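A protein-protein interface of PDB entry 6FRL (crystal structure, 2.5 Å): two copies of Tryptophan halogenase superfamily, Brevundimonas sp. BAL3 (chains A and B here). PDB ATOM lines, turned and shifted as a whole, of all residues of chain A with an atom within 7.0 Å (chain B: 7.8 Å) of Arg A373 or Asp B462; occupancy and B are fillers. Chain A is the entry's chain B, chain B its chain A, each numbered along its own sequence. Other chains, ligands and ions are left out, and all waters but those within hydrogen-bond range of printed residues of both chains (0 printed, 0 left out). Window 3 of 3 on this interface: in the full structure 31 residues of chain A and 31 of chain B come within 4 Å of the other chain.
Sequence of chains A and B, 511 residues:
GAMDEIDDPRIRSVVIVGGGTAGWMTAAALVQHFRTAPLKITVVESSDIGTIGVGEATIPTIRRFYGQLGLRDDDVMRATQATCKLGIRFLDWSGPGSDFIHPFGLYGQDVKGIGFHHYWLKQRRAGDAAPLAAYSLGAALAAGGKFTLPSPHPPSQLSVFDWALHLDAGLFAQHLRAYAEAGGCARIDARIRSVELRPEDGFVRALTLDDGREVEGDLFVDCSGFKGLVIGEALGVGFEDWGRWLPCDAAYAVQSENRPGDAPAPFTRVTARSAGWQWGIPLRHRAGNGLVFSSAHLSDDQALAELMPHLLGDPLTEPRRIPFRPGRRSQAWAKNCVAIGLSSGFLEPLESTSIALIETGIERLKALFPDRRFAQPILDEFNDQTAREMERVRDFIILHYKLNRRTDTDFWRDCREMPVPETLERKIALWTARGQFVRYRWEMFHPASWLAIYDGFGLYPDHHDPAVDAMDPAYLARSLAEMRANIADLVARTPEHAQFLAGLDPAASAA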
ATOM      1  N   PRO A   9     -12.264 -12.524 -10.769  1.00  0.00           N
ATOM      2  CA  PRO A   9     -13.731 -12.589 -10.674  1.00  0.00           C
ATOM      3  C   PRO A   9     -14.417 -13.539 -11.705  1.00  0.00           C
ATOM      4  O   PRO A   9     -15.560 -13.863 -11.538  1.00  0.00           O
ATOM      5  CB  PRO A   9     -14.163 -11.134 -10.841  1.00  0.00           C
ATOM      6  CG  PRO A   9     -12.996 -10.428 -11.451  1.00  0.00           C
ATOM      7  CD  PRO A   9     -11.821 -11.335 -11.517  1.00  0.00           C
ATOM      8  N   ARG A  10     -13.719 -13.919 -12.774  1.00  0.00           N
ATOM      9  CA  ARG A  10     -14.026 -15.057 -13.661  1.00  0.00           C
ATOM     10  C   ARG A  10     -15.079 -16.083 -13.173  1.00  0.00           C
ATOM     11  O   ARG A  10     -14.933 -16.676 -12.095  1.00  0.00           O
ATOM     12  CB  ARG A  10     -12.695 -15.812 -13.928  1.00  0.00           C
ATOM     13  CG  ARG A  10     -12.626 -16.605 -15.219  1.00  0.00           C
ATOM     14  CD  ARG A  10     -11.336 -17.451 -15.322  1.00  0.00           C
ATOM     15  NE  ARG A  10     -10.105 -16.680 -15.543  1.00  0.00           N
ATOM     16  CZ  ARG A  10      -9.808 -15.995 -16.653  1.00  0.00           C
ATOM     17  NH1 ARG A  10     -10.649 -15.949 -17.690  1.00  0.00           N
ATOM     18  NH2 ARG A  10      -8.652 -15.334 -16.737  1.00  0.00           N
ATOM     19  N   ILE A  11     -16.125 -16.301 -13.980  1.00  0.00           N
ATOM     20  CA  ILE A  11     -17.051 -17.451 -13.779  1.00  0.00           C
ATOM     21  C   ILE A  11     -16.258 -18.769 -13.976  1.00  0.00           C
ATOM     22  O   ILE A  11     -15.591 -18.960 -15.006  1.00  0.00           O
ATOM     23  CB  ILE A  11     -18.272 -17.441 -14.770  1.00  0.00           C
ATOM     24  CG1 ILE A  11     -19.121 -16.161 -14.647  1.00  0.00           C
ATOM     25  CG2 ILE A  11     -19.168 -18.662 -14.574  1.00  0.00           C
ATOM     26  CD1 ILE A  11     -19.924 -16.046 -13.373  1.00  0.00           C
ATOM     27  N   PHE A 203     -28.053 -15.179  -3.544  1.00  0.00           N
ATOM     28  CA  PHE A 203     -27.704 -15.766  -4.842  1.00  0.00           C
ATOM     29  C   PHE A 203     -27.873 -17.275  -4.725  1.00  0.00           C
ATOM     30  O   PHE A 203     -27.926 -17.794  -3.609  1.00  0.00           O
ATOM     31  CB  PHE A 203     -26.259 -15.422  -5.261  1.00  0.00           C
ATOM     32  CG  PHE A 203     -26.110 -14.087  -5.964  1.00  0.00           C
ATOM     33  CD1 PHE A 203     -26.784 -12.939  -5.535  1.00  0.00           C
ATOM     34  CD2 PHE A 203     -25.230 -13.958  -7.024  1.00  0.00           C
ATOM     35  CE1 PHE A 203     -26.588 -11.701  -6.163  1.00  0.00           C
ATOM     36  CE2 PHE A 203     -25.036 -12.727  -7.654  1.00  0.00           C
ATOM     37  CZ  PHE A 203     -25.716 -11.597  -7.229  1.00  0.00           C
ATOM     38  N   PRO A 370     -21.421 -12.670 -17.944  1.00  0.00           N
ATOM     39  CA  PRO A 370     -20.991 -11.923 -16.777  1.00  0.00           C
ATOM     40  C   PRO A 370     -19.715 -12.480 -16.127  1.00  0.00           C
ATOM     41  O   PRO A 370     -19.215 -13.530 -16.529  1.00  0.00           O
ATOM     42  CB  PRO A 370     -22.171 -12.145 -15.814  1.00  0.00           C
ATOM     43  CG  PRO A 370     -22.556 -13.571 -16.075  1.00  0.00           C
ATOM     44  CD  PRO A 370     -22.327 -13.781 -17.570  1.00  0.00           C
ATOM     45  N   ASP A 371     -19.215 -11.745 -15.132  1.00  0.00           N
ATOM     46  CA  ASP A 371     -18.342 -12.278 -14.103  1.00  0.00           C
ATOM     47  C   ASP A 371     -19.109 -12.394 -12.748  1.00  0.00           C
ATOM     48  O   ASP A 371     -20.340 -12.163 -12.672  1.00  0.00           O
ATOM     49  CB  ASP A 371     -17.031 -11.484 -14.001  1.00  0.00           C
ATOM     50  CG  ASP A 371     -17.197 -10.099 -13.397  1.00  0.00           C
ATOM     51  OD1 ASP A 371     -18.223  -9.787 -12.703  1.00  0.00           O
ATOM     52  OD2 ASP A 371     -16.278  -9.308 -13.650  1.00  0.00           O
ATOM     53  N   ARG A 372     -18.382 -12.788 -11.695  1.00  0.00           N
ATOM     54  CA  ARG A 372     -18.984 -13.158 -10.424  1.00  0.00           C
ATOM     55  C   ARG A 372     -19.503 -11.998  -9.609  1.00  0.00           C
ATOM     56  O   ARG A 372     -20.200 -12.245  -8.624  1.00  0.00           O
ATOM     57  CB  ARG A 372     -18.019 -13.990  -9.597  1.00  0.00           C
ATOM     58  CG  ARG A 372     -17.827 -15.396 -10.169  1.00  0.00           C
ATOM     59  CD  ARG A 372     -16.639 -16.090  -9.549  1.00  0.00           C
ATOM     60  NE  ARG A 372     -16.740 -16.111  -8.110  1.00  0.00           N
ATOM     61  CZ  ARG A 372     -15.749 -16.436  -7.283  1.00  0.00           C
ATOM     62  NH1 ARG A 372     -14.565 -16.790  -7.742  1.00  0.00           N
ATOM     63  NH2 ARG A 372     -15.949 -16.415  -5.972  1.00  0.00           N
ATOM     64  N   ARG A 373     -19.167 -10.771 -10.018  1.00  0.00           N
ATOM     65  CA  ARG A 373     -19.765  -9.552  -9.465  1.00  0.00           C
ATOM     66  C   ARG A 373     -21.181  -9.288  -9.965  1.00  0.00           C
ATOM     67  O   ARG A 373     -21.902  -8.505  -9.343  1.00  0.00           O
ATOM     68  CB  ARG A 373     -18.906  -8.302  -9.769  1.00  0.00           C
ATOM     69  CG  ARG A 373     -17.481  -8.368  -9.248  1.00  0.00           C
ATOM     70  CD  ARG A 373     -16.805  -6.994  -9.290  1.00  0.00           C
ATOM     71  NE  ARG A 373     -16.869  -6.307 -10.587  1.00  0.00           N
ATOM     72  CZ  ARG A 373     -16.200  -6.657 -11.695  1.00  0.00           C
ATOM     73  NH1 ARG A 373     -15.427  -7.737 -11.723  1.00  0.00           N
ATOM     74  NH2 ARG A 373     -16.334  -5.932 -12.810  1.00  0.00           N
ATOM     75  N   PHE A 374     -21.565  -9.891 -11.099  1.00  0.00           N
ATOM     76  CA  PHE A 374     -22.916  -9.758 -11.657  1.00  0.00           C
ATOM     77  C   PHE A 374     -23.397  -8.296 -11.673  1.00  0.00           C
ATOM     78  O   PHE A 374     -24.459  -7.931 -11.116  1.00  0.00           O
ATOM     79  CB  PHE A 374     -23.888 -10.712 -10.928  1.00  0.00           C
ATOM     80  CG  PHE A 374     -23.741 -12.150 -11.339  1.00  0.00           C
ATOM     81  CD1 PHE A 374     -22.829 -12.992 -10.681  1.00  0.00           C
ATOM     82  CD2 PHE A 374     -24.486 -12.666 -12.411  1.00  0.00           C
ATOM     83  CE1 PHE A 374     -22.670 -14.320 -11.070  1.00  0.00           C
ATOM     84  CE2 PHE A 374     -24.332 -13.995 -12.810  1.00  0.00           C
ATOM     85  CZ  PHE A 374     -23.407 -14.821 -12.137  1.00  0.00           C
ATOM     86  N   ALA A 375     -22.588  -7.468 -12.332  1.00  0.00           N
ATOM     87  CA  ALA A 375     -22.836  -6.039 -12.456  1.00  0.00           C
ATOM     88  C   ALA A 375     -24.257  -5.741 -12.957  1.00  0.00           C
ATOM     89  O   ALA A 375     -24.715  -6.288 -13.970  1.00  0.00           O
ATOM     90  CB  ALA A 375     -21.815  -5.430 -13.367  1.00  0.00           C
ATOM     91  N   GLN A 376     -24.946  -4.871 -12.228  1.00  0.00           N
ATOM     92  CA  GLN A 376     -26.365  -4.586 -12.439  1.00  0.00           C
ATOM     93  C   GLN A 376     -26.691  -4.108 -13.850  1.00  0.00           C
ATOM     94  O   GLN A 376     -27.726  -4.501 -14.375  1.00  0.00           O
ATOM     95  CB  GLN A 376     -26.911  -3.578 -11.380  1.00  0.00           C
ATOM     96  CG  GLN A 376     -28.441  -3.438 -11.304  1.00  0.00           C
ATOM     97  CD  GLN A 376     -29.188  -4.745 -11.092  1.00  0.00           C
ATOM     98  OE1 GLN A 376     -28.933  -5.427 -10.141  1.00  0.00           O
ATOM     99  NE2 GLN A 376     -30.113  -5.084 -11.973  1.00  0.00           N
ATOM    100  N   LEU A 379     -27.327  -7.130 -16.197  1.00  0.00           N
ATOM    101  CA  LEU A 379     -28.667  -7.698 -16.000  1.00  0.00           C
ATOM    102  C   LEU A 379     -29.730  -6.790 -16.654  1.00  0.00           C
ATOM    103  O   LEU A 379     -30.614  -7.270 -17.383  1.00  0.00           O
ATOM    104  CB  LEU A 379     -28.982  -7.904 -14.527  1.00  0.00           C
ATOM    105  CG  LEU A 379     -28.428  -9.192 -13.917  1.00  0.00           C
ATOM    106  CD1 LEU A 379     -26.912  -9.234 -13.936  1.00  0.00           C
ATOM    107  CD2 LEU A 379     -28.922  -9.315 -12.471  1.00  0.00           C
ATOM    108  N   LEU B 121      -8.137  -5.307 -25.388  1.00  0.00           N
ATOM    109  CA  LEU B 121      -8.093  -5.092 -23.943  1.00  0.00           C
ATOM    110  C   LEU B 121      -7.368  -6.203 -23.166  1.00  0.00           C
ATOM    111  O   LEU B 121      -6.584  -5.897 -22.261  1.00  0.00           O
ATOM    112  CB  LEU B 121      -9.491  -4.882 -23.370  1.00  0.00           C
ATOM    113  CG  LEU B 121     -10.101  -3.524 -23.710  1.00  0.00           C
ATOM    114  CD1 LEU B 121     -11.629  -3.585 -23.602  1.00  0.00           C
ATOM    115  CD2 LEU B 121      -9.500  -2.455 -22.815  1.00  0.00           C
ATOM    116  N   ARG B 125      -4.055  -5.646 -20.984  1.00  0.00           N
ATOM    117  CA  ARG B 125      -3.999  -6.069 -19.584  1.00  0.00           C
ATOM    118  C   ARG B 125      -2.654  -6.768 -19.317  1.00  0.00           C
ATOM    119  O   ARG B 125      -2.008  -6.514 -18.309  1.00  0.00           O
ATOM    120  CB  ARG B 125      -5.186  -7.005 -19.259  1.00  0.00           C
ATOM    121  CG  ARG B 125      -5.877  -6.698 -17.943  1.00  0.00           C
ATOM    122  CD  ARG B 125      -7.047  -7.639 -17.656  1.00  0.00           C
ATOM    123  NE  ARG B 125      -8.148  -6.952 -16.972  1.00  0.00           N
ATOM    124  CZ  ARG B 125      -8.168  -6.594 -15.680  1.00  0.00           C
ATOM    125  NH1 ARG B 125      -7.142  -6.844 -14.858  1.00  0.00           N
ATOM    126  NH2 ARG B 125      -9.241  -5.967 -15.199  1.00  0.00           N
ATOM    127  N   ALA B 429     -22.647   3.246 -18.424  1.00  0.00           N
ATOM    128  CA  ALA B 429     -22.649   2.178 -17.405  1.00  0.00           C
ATOM    129  C   ALA B 429     -22.413   0.772 -18.010  1.00  0.00           C
ATOM    130  O   ALA B 429     -21.668  -0.031 -17.432  1.00  0.00           O
ATOM    131  CB  ALA B 429     -23.932   2.213 -16.561  1.00  0.00           C
ATOM    132  N   TRP B 431     -20.885   0.190 -20.854  1.00  0.00           N
ATOM    133  CA  TRP B 431     -19.533   0.193 -21.423  1.00  0.00           C
ATOM    134  C   TRP B 431     -18.522  -0.150 -20.331  1.00  0.00           C
ATOM    135  O   TRP B 431     -17.727  -1.092 -20.512  1.00  0.00           O
ATOM    136  CB  TRP B 431     -19.174   1.526 -22.062  1.00  0.00           C
ATOM    137  CG  TRP B 431     -17.726   1.613 -22.428  1.00  0.00           C
ATOM    138  CD1 TRP B 431     -16.770   2.345 -21.800  1.00  0.00           C
ATOM    139  CD2 TRP B 431     -17.053   0.877 -23.471  1.00  0.00           C
ATOM    140  NE1 TRP B 431     -15.540   2.140 -22.418  1.00  0.00           N
ATOM    141  CE2 TRP B 431     -15.695   1.240 -23.434  1.00  0.00           C
ATOM    142  CE3 TRP B 431     -17.479  -0.057 -24.429  1.00  0.00           C
ATOM    143  CZ2 TRP B 431     -14.754   0.710 -24.306  1.00  0.00           C
ATOM    144  CZ3 TRP B 431     -16.531  -0.588 -25.314  1.00  0.00           C
ATOM    145  CH2 TRP B 431     -15.182  -0.197 -25.243  1.00  0.00           C
ATOM    146  N   THR B 432     -18.571   0.559 -19.189  1.00  0.00           N
ATOM    147  CA  THR B 432     -17.589   0.329 -18.106  1.00  0.00           C
ATOM    148  C   THR B 432     -17.769  -1.031 -17.417  1.00  0.00           C
ATOM    149  O   THR B 432     -16.812  -1.629 -16.997  1.00  0.00           O
ATOM    150  CB  THR B 432     -17.558   1.462 -17.045  1.00  0.00           C
ATOM    151  OG1 THR B 432     -18.641   1.308 -16.157  1.00  0.00           O
ATOM    152  CG2 THR B 432     -17.639   2.875 -17.666  1.00  0.00           C
ATOM    153  N   ALA B 433     -18.998  -1.531 -17.353  1.00  0.00           N
ATOM    154  CA  ALA B 433     -19.268  -2.848 -16.792  1.00  0.00           C
ATOM    155  C   ALA B 433     -18.851  -3.994 -17.674  1.00  0.00           C
ATOM    156  O   ALA B 433     -18.481  -5.032 -17.165  1.00  0.00           O
ATOM    157  CB  ALA B 433     -20.756  -2.999 -16.477  1.00  0.00           C
ATOM    158  N   ARG B 434     -18.998  -3.861 -18.979  1.00  0.00           N
ATOM    159  CA  ARG B 434     -18.931  -5.055 -19.838  1.00  0.00           C
ATOM    160  C   ARG B 434     -18.306  -4.881 -21.234  1.00  0.00           C
ATOM    161  O   ARG B 434     -18.063  -5.892 -21.921  1.00  0.00           O
ATOM    162  CB  ARG B 434     -20.346  -5.630 -19.922  1.00  0.00           C
ATOM    163  CG  ARG B 434     -20.553  -6.964 -20.627  1.00  0.00           C
ATOM    164  CD  ARG B 434     -19.620  -8.071 -20.157  1.00  0.00           C
ATOM    165  NE  ARG B 434     -19.766  -9.286 -20.949  1.00  0.00           N
ATOM    166  CZ  ARG B 434     -19.348  -9.453 -22.214  1.00  0.00           C
ATOM    167  NH1 ARG B 434     -18.754  -8.475 -22.877  1.00  0.00           N
ATOM    168  NH2 ARG B 434     -19.523 -10.630 -22.829  1.00  0.00           N
ATOM    169  N   GLY B 435     -17.998  -3.640 -21.638  1.00  0.00           N
ATOM    170  CA  GLY B 435     -17.488  -3.367 -22.977  1.00  0.00           C
ATOM    171  C   GLY B 435     -18.463  -3.612 -24.138  1.00  0.00           C
ATOM    172  O   GLY B 435     -18.053  -4.013 -25.244  1.00  0.00           O
ATOM    173  N   LEU B 459     -11.323   5.831 -21.103  1.00  0.00           N
ATOM    174  CA  LEU B 459     -12.299   5.080 -20.292  1.00  0.00           C
ATOM    175  C   LEU B 459     -12.476   3.660 -20.834  1.00  0.00           C
ATOM    176  O   LEU B 459     -13.037   3.467 -21.896  1.00  0.00           O
ATOM    177  CB  LEU B 459     -13.640   5.802 -20.247  1.00  0.00           C
ATOM    178  CG  LEU B 459     -14.740   5.126 -19.428  1.00  0.00           C
ATOM    179  CD1 LEU B 459     -14.358   5.088 -17.947  1.00  0.00           C
ATOM    180  CD2 LEU B 459     -16.102   5.803 -19.649  1.00  0.00           C
ATOM    181  N   TYR B 460     -12.030   2.675 -20.057  1.00  0.00           N
ATOM    182  CA  TYR B 460     -12.002   1.275 -20.465  1.00  0.00           C
ATOM    183  C   TYR B 460     -12.752   0.411 -19.474  1.00  0.00           C
ATOM    184  O   TYR B 460     -12.812   0.748 -18.311  1.00  0.00           O
ATOM    185  CB  TYR B 460     -10.558   0.790 -20.537  1.00  0.00           C
ATOM    186  CG  TYR B 460      -9.708   1.610 -21.491  1.00  0.00           C
ATOM    187  CD1 TYR B 460      -9.878   1.495 -22.882  1.00  0.00           C
ATOM    188  CD2 TYR B 460      -8.745   2.487 -21.027  1.00  0.00           C
ATOM    189  CE1 TYR B 460      -9.119   2.223 -23.767  1.00  0.00           C
ATOM    190  CE2 TYR B 460      -7.979   3.245 -21.914  1.00  0.00           C
ATOM    191  CZ  TYR B 460      -8.161   3.092 -23.283  1.00  0.00           C
ATOM    192  OH  TYR B 460      -7.427   3.821 -24.192  1.00  0.00           O
ATOM    193  N   PRO B 461     -13.332  -0.707 -19.939  1.00  0.00           N
ATOM    194  CA  PRO B 461     -14.073  -1.573 -19.029  1.00  0.00           C
ATOM    195  C   PRO B 461     -13.166  -2.322 -18.066  1.00  0.00           C
ATOM    196  O   PRO B 461     -12.006  -2.542 -18.376  1.00  0.00           O
ATOM    197  CB  PRO B 461     -14.788  -2.569 -19.945  1.00  0.00           C
ATOM    198  CG  PRO B 461     -14.284  -2.339 -21.307  1.00  0.00           C
ATOM    199  CD  PRO B 461     -13.583  -1.025 -21.351  1.00  0.00           C
ATOM    200  N   ASP B 462     -13.745  -2.738 -16.932  1.00  0.00           N
ATOM    201  CA  ASP B 462     -13.033  -3.500 -15.890  1.00  0.00           C
ATOM    202  C   ASP B 462     -12.831  -4.910 -16.429  1.00  0.00           C
ATOM    203  O   ASP B 462     -11.735  -5.412 -16.425  1.00  0.00           O
ATOM    204  CB  ASP B 462     -13.803  -3.576 -14.531  1.00  0.00           C
ATOM    205  CG  ASP B 462     -14.992  -2.587 -14.423  1.00  0.00           C
ATOM    206  OD1 ASP B 462     -14.805  -1.375 -14.678  1.00  0.00           O
ATOM    207  OD2 ASP B 462     -16.120  -3.018 -14.065  1.00  0.00           O
ATOM    208  N   HIS B 463     -13.927  -5.487 -16.925  1.00  0.00           N
ATOM    209  CA  HIS B 463     -14.091  -6.854 -17.437  1.00  0.00           C
ATOM    210  C   HIS B 463     -14.269  -6.904 -18.983  1.00  0.00           C
ATOM    211  O   HIS B 463     -15.304  -6.445 -19.427  1.00  0.00           O
ATOM    212  CB  HIS B 463     -15.385  -7.323 -16.704  1.00  0.00           C
ATOM    213  CG  HIS B 463     -16.037  -8.564 -17.236  1.00  0.00           C
ATOM    214  ND1 HIS B 463     -17.212  -8.538 -17.954  1.00  0.00           N
ATOM    215  CD2 HIS B 463     -15.711  -9.870 -17.104  1.00  0.00           C
ATOM    216  CE1 HIS B 463     -17.559  -9.770 -18.286  1.00  0.00           C
ATOM    217  NE2 HIS B 463     -16.675 -10.598 -17.769  1.00  0.00           N
ATOM    218  N   HIS B 464     -13.311  -7.425 -19.775  1.00  0.00           N
ATOM    219  CA  HIS B 464     -13.608  -7.788 -21.207  1.00  0.00           C
ATOM    220  C   HIS B 464     -14.417  -9.126 -21.285  1.00  0.00           C
ATOM    221  O   HIS B 464     -14.686  -9.752 -20.252  1.00  0.00           O
ATOM    222  CB  HIS B 464     -12.323  -7.843 -22.090  1.00  0.00           C
ATOM    223  CG  HIS B 464     -11.296  -8.828 -21.616  1.00  0.00           C
ATOM    224  ND1 HIS B 464     -10.162  -8.441 -20.934  1.00  0.00           N
ATOM    225  CD2 HIS B 464     -11.243 -10.182 -21.689  1.00  0.00           C
ATOM    226  CE1 HIS B 464      -9.448  -9.514 -20.622  1.00  0.00           C
ATOM    227  NE2 HIS B 464     -10.086 -10.583 -21.069  1.00  0.00           N
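O of Asp B462 is in hydrogen-bond range of NH2 of Arg B125 (2.8 Å). O of Thr B432 sits at hydrogen-bond distance from N of Asp B462. OD2 of Asp A371 is in salt-bridge range of NH1 of Arg A373 (2.6 Å).
Among the printed residues, merely in contact across the chains: Pro A370 with His B463 (3.9 Å) and Asp A371 with His B463 (3.5 Å).
Hydrophobic or aromatic side chains of chain B within 4 Å of the printed part of chain A: His B463. Printed residues of chain A that touch a printed residue of chain B: Pro A370, Asp A371 and Arg A373. Among the printed residues, Asp or Glu carboxylates within 4 Å of a Lys or Arg side-chain nitrogen of the other chain: Arg A373 with Asp B462 (3.2 Å).
Printed residues of chain B within 4 Å of Pro A370: His B463. Printed residues of chain B within 4 Å of Asp A371: His B463. Arg A373 touches just one residue of chain B: Asp B462 (3.2 Å). Tyr B460 touches none of the printed residues of chain A. Of chain A, only Arg A373 comes within 4 Å of Asp B462. Of the printed residues of chain A, His B463 touches Pro A370 (3.9 Å) and Asp A371 (3.5 Å). The nearest residue of chain B that does not touch Arg A373 is His B463 (4.2 Å).
The guanidinium group (NH2) of Arg A373 lies within salt-bridge range of the side-chain carboxylate (OD2) of Asp B462 (3.2 Å).
No position is printed for both chains.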
